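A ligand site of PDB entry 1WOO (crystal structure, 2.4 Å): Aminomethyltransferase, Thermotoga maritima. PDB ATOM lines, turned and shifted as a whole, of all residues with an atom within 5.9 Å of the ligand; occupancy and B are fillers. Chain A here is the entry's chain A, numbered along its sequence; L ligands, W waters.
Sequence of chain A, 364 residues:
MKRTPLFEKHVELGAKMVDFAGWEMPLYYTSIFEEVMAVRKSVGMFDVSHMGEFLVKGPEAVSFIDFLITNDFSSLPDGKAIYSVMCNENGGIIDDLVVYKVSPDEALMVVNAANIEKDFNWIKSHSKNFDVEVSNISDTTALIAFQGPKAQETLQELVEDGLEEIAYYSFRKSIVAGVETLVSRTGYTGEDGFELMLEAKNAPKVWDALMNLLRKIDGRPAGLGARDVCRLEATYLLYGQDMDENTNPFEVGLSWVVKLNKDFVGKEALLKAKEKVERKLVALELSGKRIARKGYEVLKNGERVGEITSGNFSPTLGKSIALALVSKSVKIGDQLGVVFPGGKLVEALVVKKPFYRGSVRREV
The side-chain carboxylate (OE1) of Glu 195 sits at hydrogen-bond distance from a nitrogen (N7) of the ligand (2.7 Å).
A nitrogen (N7) of the ligand lies within hydrogen-bond range of the side-chain hydroxyl of Tyr 100, at 2.9 Å.
N3 of the ligand lies within hydrogen-bond range of O of Val 110, 3.0 Å away.
The side-chain hydroxyl (OH) of Tyr 169 sits at hydrogen-bond distance from an oxygen (O5) of the ligand, 3.0 Å away.
N5 of the ligand lies within hydrogen-bond range of OD2 of Asp 96, 3.1 Å away.
O3 of the ligand is in salt-bridge range of NH2 of Arg 362 (3.1 Å).
An oxygen (O6) of the ligand sits at hydrogen-bond distance from the guanidinium group (NH2) of Arg 227, 3.3 Å away.
A nitrogen (N4) of the ligand lies close to the side-chain sulfur of Met 51 (3.6 Å).
The side-chain carboxylate (OE1) of Glu 195 is in hydrogen-bond range of the side-chain hydroxyl (OG1) of Thr 186, 2.5 Å away.
The backbone NH (N) of Glu 195 sits at hydrogen-bond distance from the backbone carbonyl oxygen (O) of Ser 184 (3.0 Å).
The backbone NH (N) of Val 110 sits at hydrogen-bond distance from the backbone carbonyl oxygen (O) of Val 98.
The side-chain carboxylate of Asp 96 sits at hydrogen-bond distance from the side-chain amide nitrogen of Asn 112, at 2.8 Å.
The side-chain carboxylate (OD2) of Asp 96 sits at hydrogen-bond distance from the side-chain hydroxyl (OH) of Tyr 83 (3.0 Å).
The side-chain amide nitrogen (ND2) of Asn 112 sits at hydrogen-bond distance from the side-chain carboxylate (OD2) of Asp 95 (2.7 Å).
OH of Tyr 188 is in hydrogen-bond range of O of Leu 237 (2.8 Å).
The backbone carbonyl oxygen of Gly 187 sits close to an oxygen (O5) of the ligand.
Tyr 83 touches the ligand.
Leu 97 touches the ligand.
Val 98 touches the ligand (CG2 to N2, 3.4 Å).
C of Val 111 touches C5 of the ligand, at 3.996 Å.
Asn 112 touches the ligand.
OH of Tyr 168 touches C18 of the ligand, 3.5 Å away.
CE1 of Tyr 188 touches C8 of the ligand (3.6 Å).
CE1 of Tyr 236 touches C16 of the ligand, at 3.5 Å.
CZ2 of Trp 256 touches O2 of the ligand, 3.5 Å away.
Hydrophobic or aromatic side chains within 4 Å of the ligand: Met 51, Tyr 83, Val 98, Val 110, Tyr 168, Tyr 169, Tyr 188, Tyr 236 and Trp 256.
18 residues have an atom within 4 Å of the ligand: Met 51, Tyr 83, Asp 96, Leu 97, Val 98, Tyr 100, Val 110, Val 111, Asn 112, Tyr 168, Tyr 169, Gly 187, Tyr 188, Glu 195, Arg 227, Tyr 236, Trp 256 and Arg 362.
The nearest printed residue that does not touch the ligand is Leu 237 (4.3 Å).
Water W4 lies within hydrogen-bond range of OH of Tyr 168 (2.5 Å), O5 of the ligand (2.8 Å), OH of Tyr 236 (2.9 Å) and O of Gly 187 (3.3 Å).
Water W3 lies within hydrogen-bond range of the side-chain carboxylate of Glu 195 (2.8 Å), an oxygen (O6) of the ligand (2.8 Å) and the guanidinium group of Arg 227 (2.9 Å).
Water W5 lies within hydrogen-bond range of an oxygen (O4) of the ligand (2.8 Å) and the backbone NH (N) of Tyr 83 (2.9 Å).
Water W2 bridges an oxygen (O1) of the ligand (2.9 Å) and the side-chain hydroxyl of Tyr 168 (2.9 Å).
Water W1 bridges the backbone NH (N) of Leu 237 (2.8 Å) and the side-chain hydroxyl (OH) of Tyr 83 (2.9 Å).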
ATOM      1  N   MET A  51     -19.228  -9.380  22.752  1.00  0.00           N
ATOM      2  CA  MET A  51     -19.329 -10.420  21.748  1.00  0.00           C
ATOM      3  C   MET A  51     -18.733  -9.949  20.427  1.00  0.00           C
ATOM      4  O   MET A  51     -18.599  -8.747  20.184  1.00  0.00           O
ATOM      5  CB  MET A  51     -20.783 -10.880  21.551  1.00  0.00           C
ATOM      6  CG  MET A  51     -21.361 -11.671  22.747  1.00  0.00           C
ATOM      7  SD  MET A  51     -22.799 -12.685  22.321  1.00  0.00           S
ATOM      8  CE  MET A  51     -24.031 -11.493  22.167  1.00  0.00           C
ATOM      9  N   ILE A  82     -30.219 -17.193  11.963  1.00  0.00           N
ATOM     10  CA  ILE A  82     -30.312 -18.602  12.322  1.00  0.00           C
ATOM     11  C   ILE A  82     -29.301 -19.017  13.385  1.00  0.00           C
ATOM     12  O   ILE A  82     -28.102 -18.737  13.281  1.00  0.00           O
ATOM     13  CB  ILE A  82     -30.099 -19.495  11.070  1.00  0.00           C
ATOM     14  CG1 ILE A  82     -30.331 -20.969  11.411  1.00  0.00           C
ATOM     15  CG2 ILE A  82     -28.686 -19.298  10.548  1.00  0.00           C
ATOM     16  CD1 ILE A  82     -30.273 -21.893  10.191  1.00  0.00           C
ATOM     17  N   TYR A  83     -29.774 -19.683  14.429  1.00  0.00           N
ATOM     18  CA  TYR A  83     -28.899 -20.142  15.497  1.00  0.00           C
ATOM     19  C   TYR A  83     -28.239 -21.421  15.032  1.00  0.00           C
ATOM     20  O   TYR A  83     -28.891 -22.281  14.450  1.00  0.00           O
ATOM     21  CB  TYR A  83     -29.696 -20.401  16.775  1.00  0.00           C
ATOM     22  CG  TYR A  83     -28.884 -21.058  17.861  1.00  0.00           C
ATOM     23  CD1 TYR A  83     -27.703 -20.462  18.330  1.00  0.00           C
ATOM     24  CD2 TYR A  83     -29.299 -22.259  18.429  1.00  0.00           C
ATOM     25  CE1 TYR A  83     -26.957 -21.069  19.337  1.00  0.00           C
ATOM     26  CE2 TYR A  83     -28.554 -22.875  19.431  1.00  0.00           C
ATOM     27  CZ  TYR A  83     -27.393 -22.277  19.885  1.00  0.00           C
ATOM     28  OH  TYR A  83     -26.675 -22.877  20.890  1.00  0.00           O
ATOM     29  N   ASP A  95     -17.710 -23.506  18.390  1.00  0.00           N
ATOM     30  CA  ASP A  95     -18.492 -22.451  19.020  1.00  0.00           C
ATOM     31  C   ASP A  95     -19.946 -22.547  18.547  1.00  0.00           C
ATOM     32  O   ASP A  95     -20.257 -23.271  17.589  1.00  0.00           O
ATOM     33  CB  ASP A  95     -17.929 -21.077  18.624  1.00  0.00           C
ATOM     34  CG  ASP A  95     -18.311 -19.985  19.602  1.00  0.00           C
ATOM     35  OD1 ASP A  95     -18.034 -18.811  19.292  1.00  0.00           O
ATOM     36  OD2 ASP A  95     -18.877 -20.291  20.671  1.00  0.00           O
ATOM     37  N   ASP A  96     -20.841 -21.832  19.234  1.00  0.00           N
ATOM     38  CA  ASP A  96     -22.230 -21.790  18.803  1.00  0.00           C
ATOM     39  C   ASP A  96     -22.392 -20.320  18.458  1.00  0.00           C
ATOM     40  O   ASP A  96     -21.638 -19.486  18.966  1.00  0.00           O
ATOM     41  CB  ASP A  96     -23.184 -22.257  19.912  1.00  0.00           C
ATOM     42  CG  ASP A  96     -23.260 -21.297  21.078  1.00  0.00           C
ATOM     43  OD1 ASP A  96     -22.236 -20.665  21.405  1.00  0.00           O
ATOM     44  OD2 ASP A  96     -24.346 -21.213  21.683  1.00  0.00           O
ATOM     45  N   LEU A  97     -23.333 -19.989  17.572  1.00  0.00           N
ATOM     46  CA  LEU A  97     -23.477 -18.589  17.158  1.00  0.00           C
ATOM     47  C   LEU A  97     -24.781 -18.292  16.444  1.00  0.00           C
ATOM     48  O   LEU A  97     -25.679 -19.133  16.364  1.00  0.00           O
ATOM     49  CB  LEU A  97     -22.337 -18.194  16.223  1.00  0.00           C
ATOM     50  CG  LEU A  97     -22.358 -18.836  14.815  1.00  0.00           C
ATOM     51  CD1 LEU A  97     -21.194 -18.279  13.997  1.00  0.00           C
ATOM     52  CD2 LEU A  97     -22.257 -20.367  14.906  1.00  0.00           C
ATOM     53  N   VAL A  98     -24.843 -17.085  15.906  1.00  0.00           N
ATOM     54  CA  VAL A  98     -25.993 -16.604  15.163  1.00  0.00           C
ATOM     55  C   VAL A  98     -25.481 -15.929  13.889  1.00  0.00           C
ATOM     56  O   VAL A  98     -24.630 -15.036  13.941  1.00  0.00           O
ATOM     57  CB  VAL A  98     -26.801 -15.601  15.991  1.00  0.00           C
ATOM     58  CG1 VAL A  98     -27.970 -15.054  15.163  1.00  0.00           C
ATOM     59  CG2 VAL A  98     -27.322 -16.273  17.263  1.00  0.00           C
ATOM     60  N   TYR A 100     -26.546 -13.872  10.328  1.00  0.00           N
ATOM     61  CA  TYR A 100     -27.573 -13.050   9.703  1.00  0.00           C
ATOM     62  C   TYR A 100     -27.429 -13.047   8.184  1.00  0.00           C
ATOM     63  O   TYR A 100     -26.348 -12.737   7.653  1.00  0.00           O
ATOM     64  CB  TYR A 100     -27.469 -11.606  10.222  1.00  0.00           C
ATOM     65  CG  TYR A 100     -27.559 -11.483  11.729  1.00  0.00           C
ATOM     66  CD1 TYR A 100     -28.662 -10.875  12.314  1.00  0.00           C
ATOM     67  CD2 TYR A 100     -26.548 -11.957  12.551  1.00  0.00           C
ATOM     68  CE1 TYR A 100     -28.751 -10.740  13.700  1.00  0.00           C
ATOM     69  CE2 TYR A 100     -26.627 -11.828  13.925  1.00  0.00           C
ATOM     70  CZ  TYR A 100     -27.728 -11.216  14.502  1.00  0.00           C
ATOM     71  OH  TYR A 100     -27.806 -11.082  15.866  1.00  0.00           O
ATOM     72  N   VAL A 110     -22.209 -13.614  14.587  1.00  0.00           N
ATOM     73  CA  VAL A 110     -22.046 -13.083  15.929  1.00  0.00           C
ATOM     74  C   VAL A 110     -21.653 -14.232  16.845  1.00  0.00           C
ATOM     75  O   VAL A 110     -22.412 -15.186  17.023  1.00  0.00           O
ATOM     76  CB  VAL A 110     -23.354 -12.449  16.428  1.00  0.00           C
ATOM     77  CG1 VAL A 110     -23.232 -12.041  17.892  1.00  0.00           C
ATOM     78  CG2 VAL A 110     -23.686 -11.250  15.564  1.00  0.00           C
ATOM     79  N   VAL A 111     -20.466 -14.139  17.423  1.00  0.00           N
ATOM     80  CA  VAL A 111     -19.953 -15.200  18.285  1.00  0.00           C
ATOM     81  C   VAL A 111     -19.633 -14.761  19.702  1.00  0.00           C
ATOM     82  O   VAL A 111     -19.708 -13.578  20.030  1.00  0.00           O
ATOM     83  CB  VAL A 111     -18.677 -15.790  17.664  1.00  0.00           C
ATOM     84  CG1 VAL A 111     -18.954 -16.264  16.248  1.00  0.00           C
ATOM     85  CG2 VAL A 111     -17.562 -14.732  17.676  1.00  0.00           C
ATOM     86  N   ASN A 112     -19.284 -15.749  20.523  1.00  0.00           N
ATOM     87  CA  ASN A 112     -18.941 -15.537  21.937  1.00  0.00           C
ATOM     88  C   ASN A 112     -17.607 -14.828  22.118  1.00  0.00           C
ATOM     89  O   ASN A 112     -16.636 -15.098  21.410  1.00  0.00           O
ATOM     90  CB  ASN A 112     -18.905 -16.874  22.664  1.00  0.00           C
ATOM     91  CG  ASN A 112     -20.258 -17.504  22.778  1.00  0.00           C
ATOM     92  OD1 ASN A 112     -21.152 -16.957  23.409  1.00  0.00           O
ATOM     93  ND2 ASN A 112     -20.438 -18.668  22.153  1.00  0.00           N
ATOM     94  N   LEU A 143     -23.233  -3.977  20.777  1.00  0.00           N
ATOM     95  CA  LEU A 143     -24.452  -4.770  20.714  1.00  0.00           C
ATOM     96  C   LEU A 143     -25.215  -4.656  22.028  1.00  0.00           C
ATOM     97  O   LEU A 143     -24.630  -4.799  23.092  1.00  0.00           O
ATOM     98  CB  LEU A 143     -24.102  -6.235  20.441  1.00  0.00           C
ATOM     99  CG  LEU A 143     -25.252  -7.210  20.201  1.00  0.00           C
ATOM    100  CD1 LEU A 143     -26.082  -6.724  19.030  1.00  0.00           C
ATOM    101  CD2 LEU A 143     -24.701  -8.617  19.933  1.00  0.00           C
ATOM    102  N   TYR A 168     -39.686 -13.400  14.980  1.00  0.00           N
ATOM    103  CA  TYR A 168     -38.663 -14.029  15.802  1.00  0.00           C
ATOM    104  C   TYR A 168     -37.512 -14.462  14.881  1.00  0.00           C
ATOM    105  O   TYR A 168     -37.739 -15.049  13.819  1.00  0.00           O
ATOM    106  CB  TYR A 168     -39.258 -15.245  16.520  1.00  0.00           C
ATOM    107  CG  TYR A 168     -38.329 -15.916  17.508  1.00  0.00           C
ATOM    108  CD1 TYR A 168     -37.622 -15.182  18.461  1.00  0.00           C
ATOM    109  CD2 TYR A 168     -38.186 -17.304  17.522  1.00  0.00           C
ATOM    110  CE1 TYR A 168     -36.802 -15.808  19.392  1.00  0.00           C
ATOM    111  CE2 TYR A 168     -37.378 -17.936  18.448  1.00  0.00           C
ATOM    112  CZ  TYR A 168     -36.684 -17.179  19.388  1.00  0.00           C
ATOM    113  OH  TYR A 168     -35.876 -17.815  20.300  1.00  0.00           O
ATOM    114  N   TYR A 169     -36.275 -14.181  15.283  1.00  0.00           N
ATOM    115  CA  TYR A 169     -35.097 -14.518  14.490  1.00  0.00           C
ATOM    116  C   TYR A 169     -35.114 -13.875  13.088  1.00  0.00           C
ATOM    117  O   TYR A 169     -34.734 -14.502  12.086  1.00  0.00           O
ATOM    118  CB  TYR A 169     -34.909 -16.044  14.381  1.00  0.00           C
ATOM    119  CG  TYR A 169     -33.912 -16.564  15.385  1.00  0.00           C
ATOM    120  CD1 TYR A 169     -34.228 -16.632  16.740  1.00  0.00           C
ATOM    121  CD2 TYR A 169     -32.599 -16.869  15.009  1.00  0.00           C
ATOM    122  CE1 TYR A 169     -33.275 -16.979  17.690  1.00  0.00           C
ATOM    123  CE2 TYR A 169     -31.635 -17.222  15.945  1.00  0.00           C
ATOM    124  CZ  TYR A 169     -31.989 -17.275  17.289  1.00  0.00           C
ATOM    125  OH  TYR A 169     -31.040 -17.598  18.239  1.00  0.00           O
ATOM    126  N   SER A 184     -32.803  -6.907  15.538  1.00  0.00           N
ATOM    127  CA  SER A 184     -33.233  -8.287  15.333  1.00  0.00           C
ATOM    128  C   SER A 184     -34.075  -8.741  16.518  1.00  0.00           C
ATOM    129  O   SER A 184     -33.799  -8.380  17.665  1.00  0.00           O
ATOM    130  CB  SER A 184     -32.016  -9.208  15.215  1.00  0.00           C
ATOM    131  OG  SER A 184     -31.355  -9.328  16.470  1.00  0.00           O
ATOM    132  N   THR A 186     -34.224 -11.136  18.645  1.00  0.00           N
ATOM    133  CA  THR A 186     -33.439 -12.233  19.186  1.00  0.00           C
ATOM    134  C   THR A 186     -33.096 -11.973  20.638  1.00  0.00           C
ATOM    135  O   THR A 186     -33.357 -10.894  21.171  1.00  0.00           O
ATOM    136  CB  THR A 186     -32.134 -12.395  18.410  1.00  0.00           C
ATOM    137  OG1 THR A 186     -31.419 -11.160  18.434  1.00  0.00           O
ATOM    138  CG2 THR A 186     -32.418 -12.782  16.971  1.00  0.00           C
ATOM    139  N   GLY A 187     -32.496 -12.959  21.281  1.00  0.00           N
ATOM    140  CA  GLY A 187     -32.147 -12.808  22.675  1.00  0.00           C
ATOM    141  C   GLY A 187     -31.633 -14.093  23.276  1.00  0.00           C
ATOM    142  O   GLY A 187     -31.616 -15.144  22.626  1.00  0.00           O
ATOM    143  N   TYR A 188     -31.267 -14.027  24.547  1.00  0.00           N
ATOM    144  CA  TYR A 188     -30.667 -15.156  25.251  1.00  0.00           C
ATOM    145  C   TYR A 188     -31.353 -15.287  26.610  1.00  0.00           C
ATOM    146  O   TYR A 188     -30.746 -15.726  27.587  1.00  0.00           O
ATOM    147  CB  TYR A 188     -29.181 -14.822  25.409  1.00  0.00           C
ATOM    148  CG  TYR A 188     -28.245 -15.915  25.867  1.00  0.00           C
ATOM    149  CD1 TYR A 188     -28.233 -17.175  25.253  1.00  0.00           C
ATOM    150  CD2 TYR A 188     -27.290 -15.650  26.861  1.00  0.00           C
ATOM    151  CE1 TYR A 188     -27.285 -18.135  25.601  1.00  0.00           C
ATOM    152  CE2 TYR A 188     -26.339 -16.597  27.205  1.00  0.00           C
ATOM    153  CZ  TYR A 188     -26.340 -17.834  26.578  1.00  0.00           C
ATOM    154  OH  TYR A 188     -25.383 -18.755  26.937  1.00  0.00           O
ATOM    155  N   GLU A 195     -32.190  -7.312  19.916  1.00  0.00           N
ATOM    156  CA  GLU A 195     -30.773  -7.051  20.043  1.00  0.00           C
ATOM    157  C   GLU A 195     -30.488  -5.938  19.053  1.00  0.00           C
ATOM    158  O   GLU A 195     -30.884  -6.013  17.887  1.00  0.00           O
ATOM    159  CB  GLU A 195     -29.957  -8.295  19.699  1.00  0.00           C
ATOM    160  CG  GLU A 195     -30.146  -9.437  20.682  1.00  0.00           C
ATOM    161  CD  GLU A 195     -29.111 -10.515  20.498  1.00  0.00           C
ATOM    162  OE1 GLU A 195     -29.100 -11.149  19.425  1.00  0.00           O
ATOM    163  OE2 GLU A 195     -28.293 -10.715  21.429  1.00  0.00           O
ATOM    164  N   ARG A 227     -27.837 -12.341  33.213  1.00  0.00           N
ATOM    165  CA  ARG A 227     -27.747 -12.929  31.893  1.00  0.00           C
ATOM    166  C   ARG A 227     -27.542 -14.444  32.038  1.00  0.00           C
ATOM    167  O   ARG A 227     -28.182 -15.248  31.338  1.00  0.00           O
ATOM    168  CB  ARG A 227     -26.581 -12.316  31.118  1.00  0.00           C
ATOM    169  CG  ARG A 227     -26.352 -12.911  29.718  1.00  0.00           C
ATOM    170  CD  ARG A 227     -25.229 -12.174  28.990  1.00  0.00           C
ATOM    171  NE  ARG A 227     -24.833 -12.807  27.732  1.00  0.00           N
ATOM    172  CZ  ARG A 227     -25.512 -12.727  26.591  1.00  0.00           C
ATOM    173  NH1 ARG A 227     -26.644 -12.042  26.518  1.00  0.00           N
ATOM    174  NH2 ARG A 227     -25.048 -13.329  25.515  1.00  0.00           N
ATOM    175  N   TYR A 236     -30.550 -22.364  27.638  1.00  0.00           N
ATOM    176  CA  TYR A 236     -29.715 -22.171  26.459  1.00  0.00           C
ATOM    177  C   TYR A 236     -28.313 -22.552  26.917  1.00  0.00           C
ATOM    178  O   TYR A 236     -27.977 -22.426  28.098  1.00  0.00           O
ATOM    179  CB  TYR A 236     -29.737 -20.712  25.999  1.00  0.00           C
ATOM    180  CG  TYR A 236     -31.095 -20.229  25.571  1.00  0.00           C
ATOM    181  CD1 TYR A 236     -32.035 -21.113  25.020  1.00  0.00           C
ATOM    182  CD2 TYR A 236     -31.444 -18.883  25.686  1.00  0.00           C
ATOM    183  CE1 TYR A 236     -33.286 -20.655  24.613  1.00  0.00           C
ATOM    184  CE2 TYR A 236     -32.684 -18.422  25.272  1.00  0.00           C
ATOM    185  CZ  TYR A 236     -33.596 -19.315  24.744  1.00  0.00           C
ATOM    186  OH  TYR A 236     -34.824 -18.848  24.335  1.00  0.00           O
ATOM    187  N   LEU A 237     -27.493 -23.024  25.987  1.00  0.00           N
ATOM    188  CA  LEU A 237     -26.154 -23.437  26.344  1.00  0.00           C
ATOM    189  C   LEU A 237     -25.128 -22.312  26.397  1.00  0.00           C
ATOM    190  O   LEU A 237     -25.290 -21.276  25.746  1.00  0.00           O
ATOM    191  CB  LEU A 237     -25.673 -24.537  25.384  1.00  0.00           C
ATOM    192  CG  LEU A 237     -26.664 -25.685  25.176  1.00  0.00           C
ATOM    193  CD1 LEU A 237     -25.953 -26.806  24.425  1.00  0.00           C
ATOM    194  CD2 LEU A 237     -27.219 -26.191  26.520  1.00  0.00           C
ATOM    195  N   TRP A 256     -31.096 -30.665  16.438  1.00  0.00           N
ATOM    196  CA  TRP A 256     -31.957 -29.866  15.569  1.00  0.00           C
ATOM    197  C   TRP A 256     -31.283 -28.767  14.758  1.00  0.00           C
ATOM    198  O   TRP A 256     -31.876 -28.276  13.789  1.00  0.00           O
ATOM    199  CB  TRP A 256     -33.131 -29.277  16.373  1.00  0.00           C
ATOM    200  CG  TRP A 256     -32.755 -28.249  17.394  1.00  0.00           C
ATOM    201  CD1 TRP A 256     -32.299 -28.474  18.664  1.00  0.00           C
ATOM    202  CD2 TRP A 256     -32.828 -26.824  17.251  1.00  0.00           C
ATOM    203  NE1 TRP A 256     -32.094 -27.286  19.319  1.00  0.00           N
ATOM    204  CE2 TRP A 256     -32.409 -26.254  18.471  1.00  0.00           C
ATOM    205  CE3 TRP A 256     -33.218 -25.972  16.197  1.00  0.00           C
ATOM    206  CZ2 TRP A 256     -32.360 -24.864  18.683  1.00  0.00           C
ATOM    207  CZ3 TRP A 256     -33.171 -24.591  16.404  1.00  0.00           C
ATOM    208  CH2 TRP A 256     -32.740 -24.049  17.646  1.00  0.00           C
ATOM    209  N   ARG A 362     -42.130 -17.524  18.473  1.00  0.00           N
ATOM    210  CA  ARG A 362     -41.953 -18.627  17.551  1.00  0.00           C
ATOM    211  C   ARG A 362     -41.284 -19.828  18.172  1.00  0.00           C
ATOM    212  O   ARG A 362     -41.842 -20.467  19.062  1.00  0.00           O
ATOM    213  CB  ARG A 362     -41.178 -18.116  16.336  1.00  0.00           C
ATOM    214  CG  ARG A 362     -40.440 -19.155  15.497  1.00  0.00           C
ATOM    215  CD  ARG A 362     -39.428 -18.463  14.547  1.00  0.00           C
ATOM    216  NE  ARG A 362     -38.545 -19.421  13.875  1.00  0.00           N
ATOM    217  CZ  ARG A 362     -37.219 -19.360  13.955  1.00  0.00           C
ATOM    218  NH1 ARG A 362     -36.434 -20.240  13.328  1.00  0.00           N
ATOM    219  NH2 ARG A 362     -36.645 -18.402  14.679  1.00  0.00           N
HETATM  220  N1  LIG L   1     -26.989 -13.101  20.635  1.00  0.00           N
HETATM  221  C1  LIG L   1     -26.490 -13.152  19.334  1.00  0.00           C
HETATM  222  N2  LIG L   1     -25.483 -13.987  18.987  1.00  0.00           N
HETATM  223  C2  LIG L   1     -24.874 -14.825  19.898  1.00  0.00           C
HETATM  224  C3  LIG L   1     -25.333 -14.866  21.319  1.00  0.00           C
HETATM  225  C4  LIG L   1     -26.470 -13.900  21.652  1.00  0.00           C
HETATM  226  N3  LIG L   1     -23.836 -15.696  19.561  1.00  0.00           N
HETATM  227  C5  LIG L   1     -23.085 -16.642  20.419  1.00  0.00           C
HETATM  228  C6  LIG L   1     -23.909 -17.047  21.693  1.00  0.00           C
HETATM  229  N4  LIG L   1     -24.604 -15.813  22.207  1.00  0.00           N
HETATM  230  C7  LIG L   1     -24.903 -18.147  21.267  1.00  0.00           C
HETATM  231  N5  LIG L   1     -25.778 -18.600  22.342  1.00  0.00           N
HETATM  232  C8  LIG L   1     -27.112 -18.732  22.105  1.00  0.00           C
HETATM  233  C9  LIG L   1     -27.819 -19.937  22.528  1.00  0.00           C
HETATM  234  C10 LIG L   1     -29.240 -20.091  22.261  1.00  0.00           C
HETATM  235  C11 LIG L   1     -29.944 -19.043  21.573  1.00  0.00           C
HETATM  236  C12 LIG L   1     -29.230 -17.845  21.159  1.00  0.00           C
HETATM  237  C13 LIG L   1     -27.850 -17.689  21.418  1.00  0.00           C
HETATM  238  C14 LIG L   1     -31.417 -19.100  21.221  1.00  0.00           C
HETATM  239  N6  LIG L   1     -32.013 -20.329  21.144  1.00  0.00           N
HETATM  240  C15 LIG L   1     -33.416 -20.557  20.795  1.00  0.00           C
HETATM  241  C16 LIG L   1     -33.820 -21.913  21.361  1.00  0.00           C
HETATM  242  O1  LIG L   1     -34.966 -22.163  21.713  1.00  0.00           O
HETATM  243  O2  LIG L   1     -32.882 -22.851  21.475  1.00  0.00           O
HETATM  244  C17 LIG L   1     -33.401 -20.501  19.254  1.00  0.00           C
HETATM  245  C18 LIG L   1     -34.755 -20.698  18.595  1.00  0.00           C
HETATM  246  C19 LIG L   1     -34.730 -20.641  17.069  1.00  0.00           C
HETATM  247  O3  LIG L   1     -35.795 -20.784  16.489  1.00  0.00           O
HETATM  248  O4  LIG L   1     -33.604 -20.438  16.362  1.00  0.00           O
HETATM  249  O5  LIG L   1     -32.062 -18.063  20.990  1.00  0.00           O
HETATM  250  O6  LIG L   1     -26.912 -13.861  22.831  1.00  0.00           O
HETATM  251  N7  LIG L   1     -27.004 -12.369  18.321  1.00  0.00           N
HETATM  252  O   HOH W   1     -28.238 -23.289  23.255  1.00  0.00           O
HETATM  253  O   HOH W   2     -37.067 -20.241  21.311  1.00  0.00           O
HETATM  254  O   HOH W   3     -28.082 -11.657  24.005  1.00  0.00           O
HETATM  255  O   HOH W   4     -34.328 -17.002  22.145  1.00  0.00           O
HETATM  256  O   HOH W   5     -32.388 -20.823  13.896  1.00  0.00           O
